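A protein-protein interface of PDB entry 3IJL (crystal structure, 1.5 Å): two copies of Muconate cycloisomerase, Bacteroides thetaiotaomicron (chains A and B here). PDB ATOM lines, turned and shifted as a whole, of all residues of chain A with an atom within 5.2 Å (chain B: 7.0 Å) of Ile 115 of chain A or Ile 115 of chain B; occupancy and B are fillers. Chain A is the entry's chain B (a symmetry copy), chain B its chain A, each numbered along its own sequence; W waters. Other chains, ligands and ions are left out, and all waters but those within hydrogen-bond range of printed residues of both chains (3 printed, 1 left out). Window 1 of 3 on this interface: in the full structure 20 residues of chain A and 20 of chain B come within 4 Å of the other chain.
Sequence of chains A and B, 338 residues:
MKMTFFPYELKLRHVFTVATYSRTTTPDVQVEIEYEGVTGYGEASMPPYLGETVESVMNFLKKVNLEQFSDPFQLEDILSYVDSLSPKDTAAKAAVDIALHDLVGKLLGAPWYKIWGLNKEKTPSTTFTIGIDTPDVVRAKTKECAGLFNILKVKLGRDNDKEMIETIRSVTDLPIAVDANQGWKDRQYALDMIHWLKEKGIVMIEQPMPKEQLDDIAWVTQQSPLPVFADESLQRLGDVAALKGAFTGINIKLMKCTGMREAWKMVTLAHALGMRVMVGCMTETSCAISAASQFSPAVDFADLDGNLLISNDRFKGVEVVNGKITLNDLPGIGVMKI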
ATOM      1  N   GLY A 105     -17.438  11.551  33.082  1.00  0.00           N
ATOM      2  CA  GLY A 105     -17.697  12.976  32.976  1.00  0.00           C
ATOM      3  C   GLY A 105     -17.446  13.656  34.309  1.00  0.00           C
ATOM      4  O   GLY A 105     -16.927  14.768  34.363  1.00  0.00           O
ATOM      5  N   LEU A 108     -13.826  14.092  34.851  1.00  0.00           N
ATOM      6  CA  LEU A 108     -13.315  15.148  33.980  1.00  0.00           C
ATOM      7  C   LEU A 108     -13.883  16.511  34.346  1.00  0.00           C
ATOM      8  O   LEU A 108     -13.361  17.539  33.917  1.00  0.00           O
ATOM      9  CB  LEU A 108     -13.666  14.856  32.522  1.00  0.00           C
ATOM     10  CG  LEU A 108     -12.822  13.828  31.779  1.00  0.00           C
ATOM     11  CD1 LEU A 108     -13.439  13.559  30.416  1.00  0.00           C
ATOM     12  CD2 LEU A 108     -11.391  14.352  31.633  1.00  0.00           C
ATOM     13  N   ALA A 110     -16.926  17.644  33.493  1.00  0.00           N
ATOM     14  CA  ALA A 110     -17.644  18.199  32.352  1.00  0.00           C
ATOM     15  C   ALA A 110     -18.809  17.325  31.900  1.00  0.00           C
ATOM     16  O   ALA A 110     -18.773  16.102  32.045  1.00  0.00           O
ATOM     17  CB  ALA A 110     -16.679  18.402  31.185  1.00  0.00           C
ATOM     18  N   PRO A 111     -19.867  17.955  31.364  1.00  0.00           N
ATOM     19  CA  PRO A 111     -21.043  17.222  30.878  1.00  0.00           C
ATOM     20  C   PRO A 111     -20.646  16.612  29.537  1.00  0.00           C
ATOM     21  O   PRO A 111     -19.780  17.149  28.845  1.00  0.00           O
ATOM     22  CB  PRO A 111     -22.094  18.316  30.685  1.00  0.00           C
ATOM     23  CG  PRO A 111     -21.609  19.459  31.535  1.00  0.00           C
ATOM     24  CD  PRO A 111     -20.119  19.403  31.374  1.00  0.00           C
ATOM     25  N   TRP A 112     -21.277  15.515  29.140  1.00  0.00           N
ATOM     26  CA  TRP A 112     -20.905  14.931  27.864  1.00  0.00           C
ATOM     27  C   TRP A 112     -21.210  15.785  26.639  1.00  0.00           C
ATOM     28  O   TRP A 112     -20.515  15.674  25.634  1.00  0.00           O
ATOM     29  CB  TRP A 112     -21.489  13.523  27.721  1.00  0.00           C
ATOM     30  CG  TRP A 112     -20.564  12.531  28.349  1.00  0.00           C
ATOM     31  CD1 TRP A 112     -20.564  12.112  29.649  1.00  0.00           C
ATOM     32  CD2 TRP A 112     -19.408  11.948  27.741  1.00  0.00           C
ATOM     33  NE1 TRP A 112     -19.472  11.312  29.891  1.00  0.00           N
ATOM     34  CE2 TRP A 112     -18.744  11.195  28.736  1.00  0.00           C
ATOM     35  CE3 TRP A 112     -18.861  11.995  26.451  1.00  0.00           C
ATOM     36  CZ2 TRP A 112     -17.562  10.491  28.479  1.00  0.00           C
ATOM     37  CZ3 TRP A 112     -17.683  11.294  26.196  1.00  0.00           C
ATOM     38  CH2 TRP A 112     -17.049  10.553  27.209  1.00  0.00           C
ATOM     39  N   TYR A 113     -22.216  16.654  26.704  1.00  0.00           N
ATOM     40  CA  TYR A 113     -22.489  17.485  25.535  1.00  0.00           C
ATOM     41  C   TYR A 113     -21.254  18.351  25.274  1.00  0.00           C
ATOM     42  O   TYR A 113     -20.905  18.630  24.126  1.00  0.00           O
ATOM     43  CB  TYR A 113     -23.740  18.364  25.746  1.00  0.00           C
ATOM     44  CG  TYR A 113     -23.532  19.611  26.589  1.00  0.00           C
ATOM     45  CD1 TYR A 113     -22.884  20.733  26.069  1.00  0.00           C
ATOM     46  CD2 TYR A 113     -23.965  19.661  27.912  1.00  0.00           C
ATOM     47  CE1 TYR A 113     -22.670  21.870  26.847  1.00  0.00           C
ATOM     48  CE2 TYR A 113     -23.756  20.800  28.699  1.00  0.00           C
ATOM     49  CZ  TYR A 113     -23.106  21.895  28.157  1.00  0.00           C
ATOM     50  OH  TYR A 113     -22.872  23.006  28.939  1.00  0.00           O
ATOM     51  N   LYS A 114     -20.579  18.745  26.353  1.00  0.00           N
ATOM     52  CA  LYS A 114     -19.388  19.587  26.263  1.00  0.00           C
ATOM     53  C   LYS A 114     -18.170  18.782  25.807  1.00  0.00           C
ATOM     54  O   LYS A 114     -17.372  19.251  24.993  1.00  0.00           O
ATOM     55  CB  LYS A 114     -19.132  20.239  27.624  1.00  0.00           C
ATOM     56  CG  LYS A 114     -18.026  21.280  27.645  1.00  0.00           C
ATOM     57  CD  LYS A 114     -17.999  21.979  29.001  1.00  0.00           C
ATOM     58  CE  LYS A 114     -16.907  23.033  29.071  1.00  0.00           C
ATOM     59  NZ  LYS A 114     -16.925  23.727  30.393  1.00  0.00           N
ATOM     60  N   ILE A 115     -18.029  17.569  26.337  1.00  0.00           N
ATOM     61  CA  ILE A 115     -16.925  16.700  25.958  1.00  0.00           C
ATOM     62  C   ILE A 115     -17.045  16.394  24.463  1.00  0.00           C
ATOM     63  O   ILE A 115     -16.041  16.345  23.740  1.00  0.00           O
ATOM     64  CB  ILE A 115     -16.959  15.383  26.778  1.00  0.00           C
ATOM     65  CG1 ILE A 115     -16.729  15.707  28.261  1.00  0.00           C
ATOM     66  CG2 ILE A 115     -15.907  14.405  26.261  1.00  0.00           C
ATOM     67  CD1 ILE A 115     -17.022  14.553  29.213  1.00  0.00           C
ATOM     68  N   TRP A 116     -18.279  16.213  23.996  1.00  0.00           N
ATOM     69  CA  TRP A 116     -18.521  15.918  22.585  1.00  0.00           C
ATOM     70  C   TRP A 116     -18.414  17.154  21.697  1.00  0.00           C
ATOM     71  O   TRP A 116     -18.525  17.054  20.472  1.00  0.00           O
ATOM     72  CB  TRP A 116     -19.894  15.265  22.390  1.00  0.00           C
ATOM     73  CG  TRP A 116     -19.947  13.808  22.771  1.00  0.00           C
ATOM     74  CD1 TRP A 116     -18.968  12.868  22.575  1.00  0.00           C
ATOM     75  CD2 TRP A 116     -21.075  13.103  23.303  1.00  0.00           C
ATOM     76  NE1 TRP A 116     -19.425  11.621  22.949  1.00  0.00           N
ATOM     77  CE2 TRP A 116     -20.714  11.738  23.398  1.00  0.00           C
ATOM     78  CE3 TRP A 116     -22.360  13.492  23.706  1.00  0.00           C
ATOM     79  CZ2 TRP A 116     -21.595  10.761  23.878  1.00  0.00           C
ATOM     80  CZ3 TRP A 116     -23.236  12.518  24.184  1.00  0.00           C
ATOM     81  CH2 TRP A 116     -22.847  11.170  24.264  1.00  0.00           C
ATOM     82  N   GLY A 117     -18.210  18.314  22.319  1.00  0.00           N
ATOM     83  CA  GLY A 117     -18.050  19.557  21.575  1.00  0.00           C
ATOM     84  C   GLY A 117     -19.315  20.175  21.008  1.00  0.00           C
ATOM     85  O   GLY A 117     -19.269  20.889  20.003  1.00  0.00           O
ATOM     86  N   PHE B  73     -14.838  24.982  23.685  1.00  0.00           N
ATOM     87  CA  PHE B  73     -15.443  23.652  23.695  1.00  0.00           C
ATOM     88  C   PHE B  73     -16.496  23.482  22.605  1.00  0.00           C
ATOM     89  O   PHE B  73     -17.004  22.383  22.395  1.00  0.00           O
ATOM     90  CB  PHE B  73     -16.054  23.355  25.070  1.00  0.00           C
ATOM     91  CG  PHE B  73     -15.038  22.959  26.107  1.00  0.00           C
ATOM     92  CD1 PHE B  73     -14.771  21.617  26.364  1.00  0.00           C
ATOM     93  CD2 PHE B  73     -14.330  23.928  26.810  1.00  0.00           C
ATOM     94  CE1 PHE B  73     -13.813  21.245  27.306  1.00  0.00           C
ATOM     95  CE2 PHE B  73     -13.368  23.565  27.754  1.00  0.00           C
ATOM     96  CZ  PHE B  73     -13.111  22.221  28.002  1.00  0.00           C
ATOM     97  N   LEU B  75     -16.484  22.863  19.650  1.00  0.00           N
ATOM     98  CA  LEU B  75     -15.783  22.307  18.498  1.00  0.00           C
ATOM     99  C   LEU B  75     -16.653  22.064  17.270  1.00  0.00           C
ATOM    100  O   LEU B  75     -16.233  22.330  16.147  1.00  0.00           O
ATOM    101  CB  LEU B  75     -15.062  21.015  18.898  1.00  0.00           C
ATOM    102  CG  LEU B  75     -13.965  21.205  19.953  1.00  0.00           C
ATOM    103  CD1 LEU B  75     -13.280  19.874  20.220  1.00  0.00           C
ATOM    104  CD2 LEU B  75     -12.950  22.236  19.473  1.00  0.00           C
ATOM    105  N   HIS B 101      -8.099  21.360  19.630  1.00  0.00           N
ATOM    106  CA  HIS B 101      -8.127  20.144  20.432  1.00  0.00           C
ATOM    107  C   HIS B 101      -7.077  20.214  21.526  1.00  0.00           C
ATOM    108  O   HIS B 101      -7.322  19.790  22.653  1.00  0.00           O
ATOM    109  CB  HIS B 101      -7.899  18.913  19.556  1.00  0.00           C
ATOM    110  CG  HIS B 101      -9.078  18.568  18.704  1.00  0.00           C
ATOM    111  ND1 HIS B 101     -10.051  17.674  19.100  1.00  0.00           N
ATOM    112  CD2 HIS B 101      -9.473  19.045  17.502  1.00  0.00           C
ATOM    113  CE1 HIS B 101     -10.992  17.617  18.174  1.00  0.00           C
ATOM    114  NE2 HIS B 101     -10.666  18.441  17.196  1.00  0.00           N
ATOM    115  N   VAL B 104      -8.589  22.523  24.195  1.00  0.00           N
ATOM    116  CA  VAL B 104      -9.672  21.877  24.932  1.00  0.00           C
ATOM    117  C   VAL B 104      -9.154  20.785  25.863  1.00  0.00           C
ATOM    118  O   VAL B 104      -9.593  20.680  27.012  1.00  0.00           O
ATOM    119  CB  VAL B 104     -10.726  21.291  23.961  1.00  0.00           C
ATOM    120  CG1 VAL B 104     -11.685  20.368  24.705  1.00  0.00           C
ATOM    121  CG2 VAL B 104     -11.501  22.428  23.313  1.00  0.00           C
ATOM    122  N   GLY B 105      -8.226  19.968  25.370  1.00  0.00           N
ATOM    123  CA  GLY B 105      -7.666  18.911  26.195  1.00  0.00           C
ATOM    124  C   GLY B 105      -6.955  19.491  27.405  1.00  0.00           C
ATOM    125  O   GLY B 105      -7.024  18.939  28.504  1.00  0.00           O
ATOM    126  N   LYS B 106      -6.263  20.608  27.205  1.00  0.00           N
ATOM    127  CA  LYS B 106      -5.561  21.259  28.305  1.00  0.00           C
ATOM    128  C   LYS B 106      -6.548  21.821  29.327  1.00  0.00           C
ATOM    129  O   LYS B 106      -6.298  21.772  30.531  1.00  0.00           O
ATOM    130  CB  LYS B 106      -4.649  22.367  27.766  1.00  0.00           C
ATOM    131  CG  LYS B 106      -3.368  21.820  27.147  1.00  0.00           C
ATOM    132  CD  LYS B 106      -2.570  22.872  26.398  1.00  0.00           C
ATOM    133  CE  LYS B 106      -1.203  22.314  26.024  1.00  0.00           C
ATOM    134  NZ  LYS B 106      -0.470  23.174  25.058  1.00  0.00           N
ATOM    135  N   LEU B 108      -9.417  20.580  29.954  1.00  0.00           N
ATOM    136  CA  LEU B 108     -10.011  19.416  30.610  1.00  0.00           C
ATOM    137  C   LEU B 108      -8.985  18.645  31.431  1.00  0.00           C
ATOM    138  O   LEU B 108      -9.343  17.799  32.251  1.00  0.00           O
ATOM    139  CB  LEU B 108     -10.614  18.463  29.576  1.00  0.00           C
ATOM    140  CG  LEU B 108     -11.977  18.802  28.981  1.00  0.00           C
ATOM    141  CD1 LEU B 108     -12.279  17.848  27.835  1.00  0.00           C
ATOM    142  CD2 LEU B 108     -13.045  18.701  30.067  1.00  0.00           C
ATOM    143  N   GLY B 109      -7.708  18.928  31.201  1.00  0.00           N
ATOM    144  CA  GLY B 109      -6.662  18.234  31.926  1.00  0.00           C
ATOM    145  C   GLY B 109      -6.528  16.780  31.501  1.00  0.00           C
ATOM    146  O   GLY B 109      -6.234  15.907  32.319  1.00  0.00           O
ATOM    147  N   ALA B 110      -6.740  16.512  30.217  1.00  0.00           N
ATOM    148  CA  ALA B 110      -6.629  15.146  29.723  1.00  0.00           C
ATOM    149  C   ALA B 110      -6.194  15.085  28.267  1.00  0.00           C
ATOM    150  O   ALA B 110      -6.487  15.986  27.480  1.00  0.00           O
ATOM    151  CB  ALA B 110      -7.968  14.423  29.885  1.00  0.00           C
ATOM    152  N   PRO B 111      -5.457  14.028  27.900  1.00  0.00           N
ATOM    153  CA  PRO B 111      -5.005  13.867  26.516  1.00  0.00           C
ATOM    154  C   PRO B 111      -6.193  13.339  25.718  1.00  0.00           C
ATOM    155  O   PRO B 111      -7.094  12.713  26.281  1.00  0.00           O
ATOM    156  CB  PRO B 111      -3.877  12.847  26.634  1.00  0.00           C
ATOM    157  CG  PRO B 111      -4.283  12.026  27.804  1.00  0.00           C
ATOM    158  CD  PRO B 111      -4.814  13.042  28.786  1.00  0.00           C
ATOM    159  N   TRP B 112      -6.215  13.583  24.414  1.00  0.00           N
ATOM    160  CA  TRP B 112      -7.342  13.111  23.638  1.00  0.00           C
ATOM    161  C   TRP B 112      -7.532  11.601  23.556  1.00  0.00           C
ATOM    162  O   TRP B 112      -8.659  11.142  23.398  1.00  0.00           O
ATOM    163  CB  TRP B 112      -7.336  13.750  22.247  1.00  0.00           C
ATOM    164  CG  TRP B 112      -8.004  15.089  22.300  1.00  0.00           C
ATOM    165  CD1 TRP B 112      -7.418  16.294  22.577  1.00  0.00           C
ATOM    166  CD2 TRP B 112      -9.411  15.337  22.230  1.00  0.00           C
ATOM    167  NE1 TRP B 112      -8.379  17.273  22.695  1.00  0.00           N
ATOM    168  CE2 TRP B 112      -9.611  16.713  22.485  1.00  0.00           C
ATOM    169  CE3 TRP B 112     -10.528  14.526  21.982  1.00  0.00           C
ATOM    170  CZ2 TRP B 112     -10.882  17.295  22.500  1.00  0.00           C
ATOM    171  CZ3 TRP B 112     -11.792  15.107  21.998  1.00  0.00           C
ATOM    172  CH2 TRP B 112     -11.957  16.481  22.255  1.00  0.00           C
ATOM    173  N   TYR B 113      -6.465  10.815  23.674  1.00  0.00           N
ATOM    174  CA  TYR B 113      -6.658   9.366  23.620  1.00  0.00           C
ATOM    175  C   TYR B 113      -7.545   8.961  24.800  1.00  0.00           C
ATOM    176  O   TYR B 113      -8.358   8.043  24.695  1.00  0.00           O
ATOM    177  CB  TYR B 113      -5.311   8.616  23.671  1.00  0.00           C
ATOM    178  CG  TYR B 113      -4.672   8.501  25.041  1.00  0.00           C
ATOM    179  CD1 TYR B 113      -5.166   7.607  25.992  1.00  0.00           C
ATOM    180  CD2 TYR B 113      -3.582   9.301  25.394  1.00  0.00           C
ATOM    181  CE1 TYR B 113      -4.599   7.517  27.259  1.00  0.00           C
ATOM    182  CE2 TYR B 113      -3.005   9.213  26.666  1.00  0.00           C
ATOM    183  CZ  TYR B 113      -3.524   8.322  27.589  1.00  0.00           C
ATOM    184  OH  TYR B 113      -2.992   8.252  28.862  1.00  0.00           O
ATOM    185  N   LYS B 114      -7.398   9.673  25.915  1.00  0.00           N
ATOM    186  CA  LYS B 114      -8.167   9.393  27.122  1.00  0.00           C
ATOM    187  C   LYS B 114      -9.593   9.923  26.994  1.00  0.00           C
ATOM    188  O   LYS B 114     -10.549   9.269  27.418  1.00  0.00           O
ATOM    189  CB  LYS B 114      -7.461  10.017  28.332  1.00  0.00           C
ATOM    190  CG  LYS B 114      -8.057   9.671  29.689  1.00  0.00           C
ATOM    191  CD  LYS B 114      -7.132  10.172  30.805  1.00  0.00           C
ATOM    192  CE  LYS B 114      -7.663   9.823  32.190  1.00  0.00           C
ATOM    193  NZ  LYS B 114      -6.739  10.306  33.260  1.00  0.00           N
ATOM    194  N   ILE B 115      -9.737  11.111  26.414  1.00  0.00           N
ATOM    195  CA  ILE B 115     -11.054  11.700  26.212  1.00  0.00           C
ATOM    196  C   ILE B 115     -11.859  10.793  25.275  1.00  0.00           C
ATOM    197  O   ILE B 115     -13.064  10.605  25.465  1.00  0.00           O
ATOM    198  CB  ILE B 115     -10.933  13.116  25.603  1.00  0.00           C
ATOM    199  CG1 ILE B 115     -10.236  14.038  26.610  1.00  0.00           C
ATOM    200  CG2 ILE B 115     -12.314  13.655  25.227  1.00  0.00           C
ATOM    201  CD1 ILE B 115      -9.858  15.397  26.050  1.00  0.00           C
ATOM    202  N   TRP B 116     -11.183  10.218  24.280  1.00  0.00           N
ATOM    203  CA  TRP B 116     -11.835   9.321  23.327  1.00  0.00           C
ATOM    204  C   TRP B 116     -12.046   7.916  23.892  1.00  0.00           C
ATOM    205  O   TRP B 116     -12.623   7.054  23.225  1.00  0.00           O
ATOM    206  CB  TRP B 116     -11.029   9.230  22.026  1.00  0.00           C
ATOM    207  CG  TRP B 116     -11.169  10.426  21.124  1.00  0.00           C
ATOM    208  CD1 TRP B 116     -12.299  11.170  20.911  1.00  0.00           C
ATOM    209  CD2 TRP B 116     -10.174  10.949  20.238  1.00  0.00           C
ATOM    210  NE1 TRP B 116     -12.067  12.122  19.943  1.00  0.00           N
ATOM    211  CE2 TRP B 116     -10.770  12.006  19.512  1.00  0.00           C
ATOM    212  CE3 TRP B 116      -8.834  10.625  19.983  1.00  0.00           C
ATOM    213  CZ2 TRP B 116     -10.070  12.742  18.545  1.00  0.00           C
ATOM    214  CZ3 TRP B 116      -8.138  11.360  19.020  1.00  0.00           C
ATOM    215  CH2 TRP B 116      -8.761  12.404  18.314  1.00  0.00           C
ATOM    216  N   GLY B 117     -11.562   7.686  25.112  1.00  0.00           N
ATOM    217  CA  GLY B 117     -11.740   6.398  25.769  1.00  0.00           C
ATOM    218  C   GLY B 117     -10.874   5.260  25.271  1.00  0.00           C
ATOM    219  O   GLY B 117     -11.258   4.092  25.364  1.00  0.00           O
ATOM    220  N   LEU B 118      -9.688   5.591  24.775  1.00  0.00           N
ATOM    221  CA  LEU B 118      -8.776   4.591  24.235  1.00  0.00           C
ATOM    222  C   LEU B 118      -7.686   4.141  25.200  1.00  0.00           C
ATOM    223  O   LEU B 118      -7.346   4.848  26.146  1.00  0.00           O
ATOM    224  CB  LEU B 118      -8.132   5.137  22.961  1.00  0.00           C
ATOM    225  CG  LEU B 118      -9.143   5.607  21.915  1.00  0.00           C
ATOM    226  CD1 LEU B 118      -8.411   6.224  20.734  1.00  0.00           C
ATOM    227  CD2 LEU B 118     -10.005   4.434  21.469  1.00  0.00           C
ATOM    228  N   ARG B 261     -10.942  16.035  14.645  1.00  0.00           N
ATOM    229  CA  ARG B 261     -12.371  15.765  14.759  1.00  0.00           C
ATOM    230  C   ARG B 261     -12.881  14.952  13.576  1.00  0.00           C
ATOM    231  O   ARG B 261     -13.586  13.961  13.763  1.00  0.00           O
ATOM    232  CB  ARG B 261     -13.165  17.071  14.903  1.00  0.00           C
ATOM    233  CG  ARG B 261     -14.626  16.862  15.310  1.00  0.00           C
ATOM    234  CD  ARG B 261     -15.267  18.179  15.733  1.00  0.00           C
ATOM    235  NE  ARG B 261     -16.665  18.042  16.147  1.00  0.00           N
ATOM    236  CZ  ARG B 261     -17.067  17.711  17.372  1.00  0.00           C
ATOM    237  NH1 ARG B 261     -16.181  17.475  18.330  1.00  0.00           N
ATOM    238  NH2 ARG B 261     -18.365  17.629  17.642  1.00  0.00           N
ATOM    239  N   GLN B 294      -2.903  10.466  18.918  1.00  0.00           N
ATOM    240  CA  GLN B 294      -3.936  10.364  19.946  1.00  0.00           C
ATOM    241  C   GLN B 294      -5.027   9.343  19.615  1.00  0.00           C
ATOM    242  O   GLN B 294      -5.672   8.821  20.522  1.00  0.00           O
ATOM    243  CB  GLN B 294      -4.568  11.731  20.222  1.00  0.00           C
ATOM    244  CG  GLN B 294      -3.631  12.766  20.869  1.00  0.00           C
ATOM    245  CD  GLN B 294      -3.122  12.359  22.244  1.00  0.00           C
ATOM    246  OE1 GLN B 294      -3.827  11.712  23.019  1.00  0.00           O
ATOM    247  NE2 GLN B 294      -1.894  12.762  22.561  1.00  0.00           N
ATOM    248  N   GLY B 332      -4.293  17.481  26.092  1.00  0.00           N
ATOM    249  CA  GLY B 332      -4.407  17.964  24.726  1.00  0.00           C
ATOM    250  C   GLY B 332      -3.825  16.985  23.729  1.00  0.00           C
ATOM    251  O   GLY B 332      -4.151  15.798  23.761  1.00  0.00           O
HETATM  252  O   HOH W   1     -11.020  18.512  34.142  1.00  0.00           O
HETATM  253  O   HOH W   2     -17.963  14.601  19.231  1.00  0.00           O
HETATM  254  O   HOH W   3     -15.298  17.045  21.167  1.00  0.00           O
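The backbone NH of Leu 75 of chain B is in hydrogen-bond range of the backbone carbonyl oxygen of Gly 117 of chain A, at 3.4 Å. NH2 of Arg 261 of chain B sits at hydrogen-bond distance from O of Trp 116 of chain A (2.9 Å).
The backbone carbonyl oxygen of Gly 105 of chain B sits at hydrogen-bond distance from the backbone NH of Ala 110 of chain B (3.0 Å). O of Ala 110 of chain B is in hydrogen-bond range of N of Gly 332 of chain B (3.0 Å). O of Gly 105 of chain A sits at hydrogen-bond distance from N of Ala 110 of chain A, 3.0 Å away.
Among the printed residues, merely in contact across the chains: Gly 117 of chain A with Phe 73 of chain B (3.1 Å), Lys 114 of chain A with Phe 73 of chain B (3.5 Å), Ile 115 of chain A with Ile 115 of chain B (3.8 Å), Ala 110 of chain A with Leu 108 of chain B (3.8 Å) and Leu 108 of chain A with Ala 110 of chain B (3.8 Å).
Of the printed residues of chain B, Ala 110 of chain A touches Leu 108. Pro 111 of chain A touches none of the printed residues of chain B. Printed residues of chain B within 4 Å of Lys 114 of chain A: Phe 73. Of the printed residues of chain B, Ile 115 of chain A touches Ile 115. Of the printed residues of chain B, Gly 117 of chain A touches Phe 73 (3.1 Å) and Leu 75 (3.4 Å). Of the printed residues of chain A, Leu 75 of chain B touches Gly 117 (3.4 Å). His 101 of chain B touches none of the printed residues of chain A. Of the printed residues of chain A, Ala 110 of chain B touches Leu 108. Printed residues of chain A within 4 Å of Ile 115 of chain B: Ile 115. The nearest printed residue of chain A that does not touch Phe 73 of chain B is Ile 115 of chain A (5.2 Å).
Printed residues of chain B that touch a printed residue of chain A: Phe 73, Leu 75, Leu 108, Ala 110, Ile 115 and Arg 261. Hydrophobic or aromatic side chains of chain B within 4 Å of the printed part of chain A: Phe 73, Leu 108, Ala 110 and Ile 115. Along chain B the printed residues that touch a printed residue of chain A span positions 73 to 261. Of the 10 printed residues of chain A, 6 touch a printed residue of chain B. Hydrophobic or aromatic side chains of chain A within 4 Å of the printed part of chain B: Leu 108, Ala 110 and Ile 115. Among the printed residues, 7 pairs touch across the chains. Among the printed residues, no Asp or Glu carboxylate lies within 4 Å of a Lys or Arg side-chain nitrogen of the other chain.
Leu 108 of chain A touches Ala 110 of chain B, and with the chains exchanged Ala 110 of chain A touches Leu 108 of chain B. Ile 115 of chain B touches its own counterpart, Ile 115 of chain A. Of the 7 pairs that touch across the chains among the printed residues, 3 have their exchanged pair printed and touching as well.
Water W1 bridges O of Leu 108 of chain A (2.5 Å) and O of Leu 108 of chain B (2.6 Å). Water W3 lies within hydrogen-bond range of the backbone carbonyl oxygen (O) of Ile 115 of chain A (2.8 Å), the guanidinium group (NH1) of Arg 261 of chain B (3.0 Å), the backbone carbonyl oxygen (O) of Trp 116 of chain A (3.3 Å) and the backbone NH (N) of Gly 117 of chain A (3.4 Å). Water W2 lies within hydrogen-bond range of O of Trp 116 of chain A and NH2 of Arg 261 of chain B.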
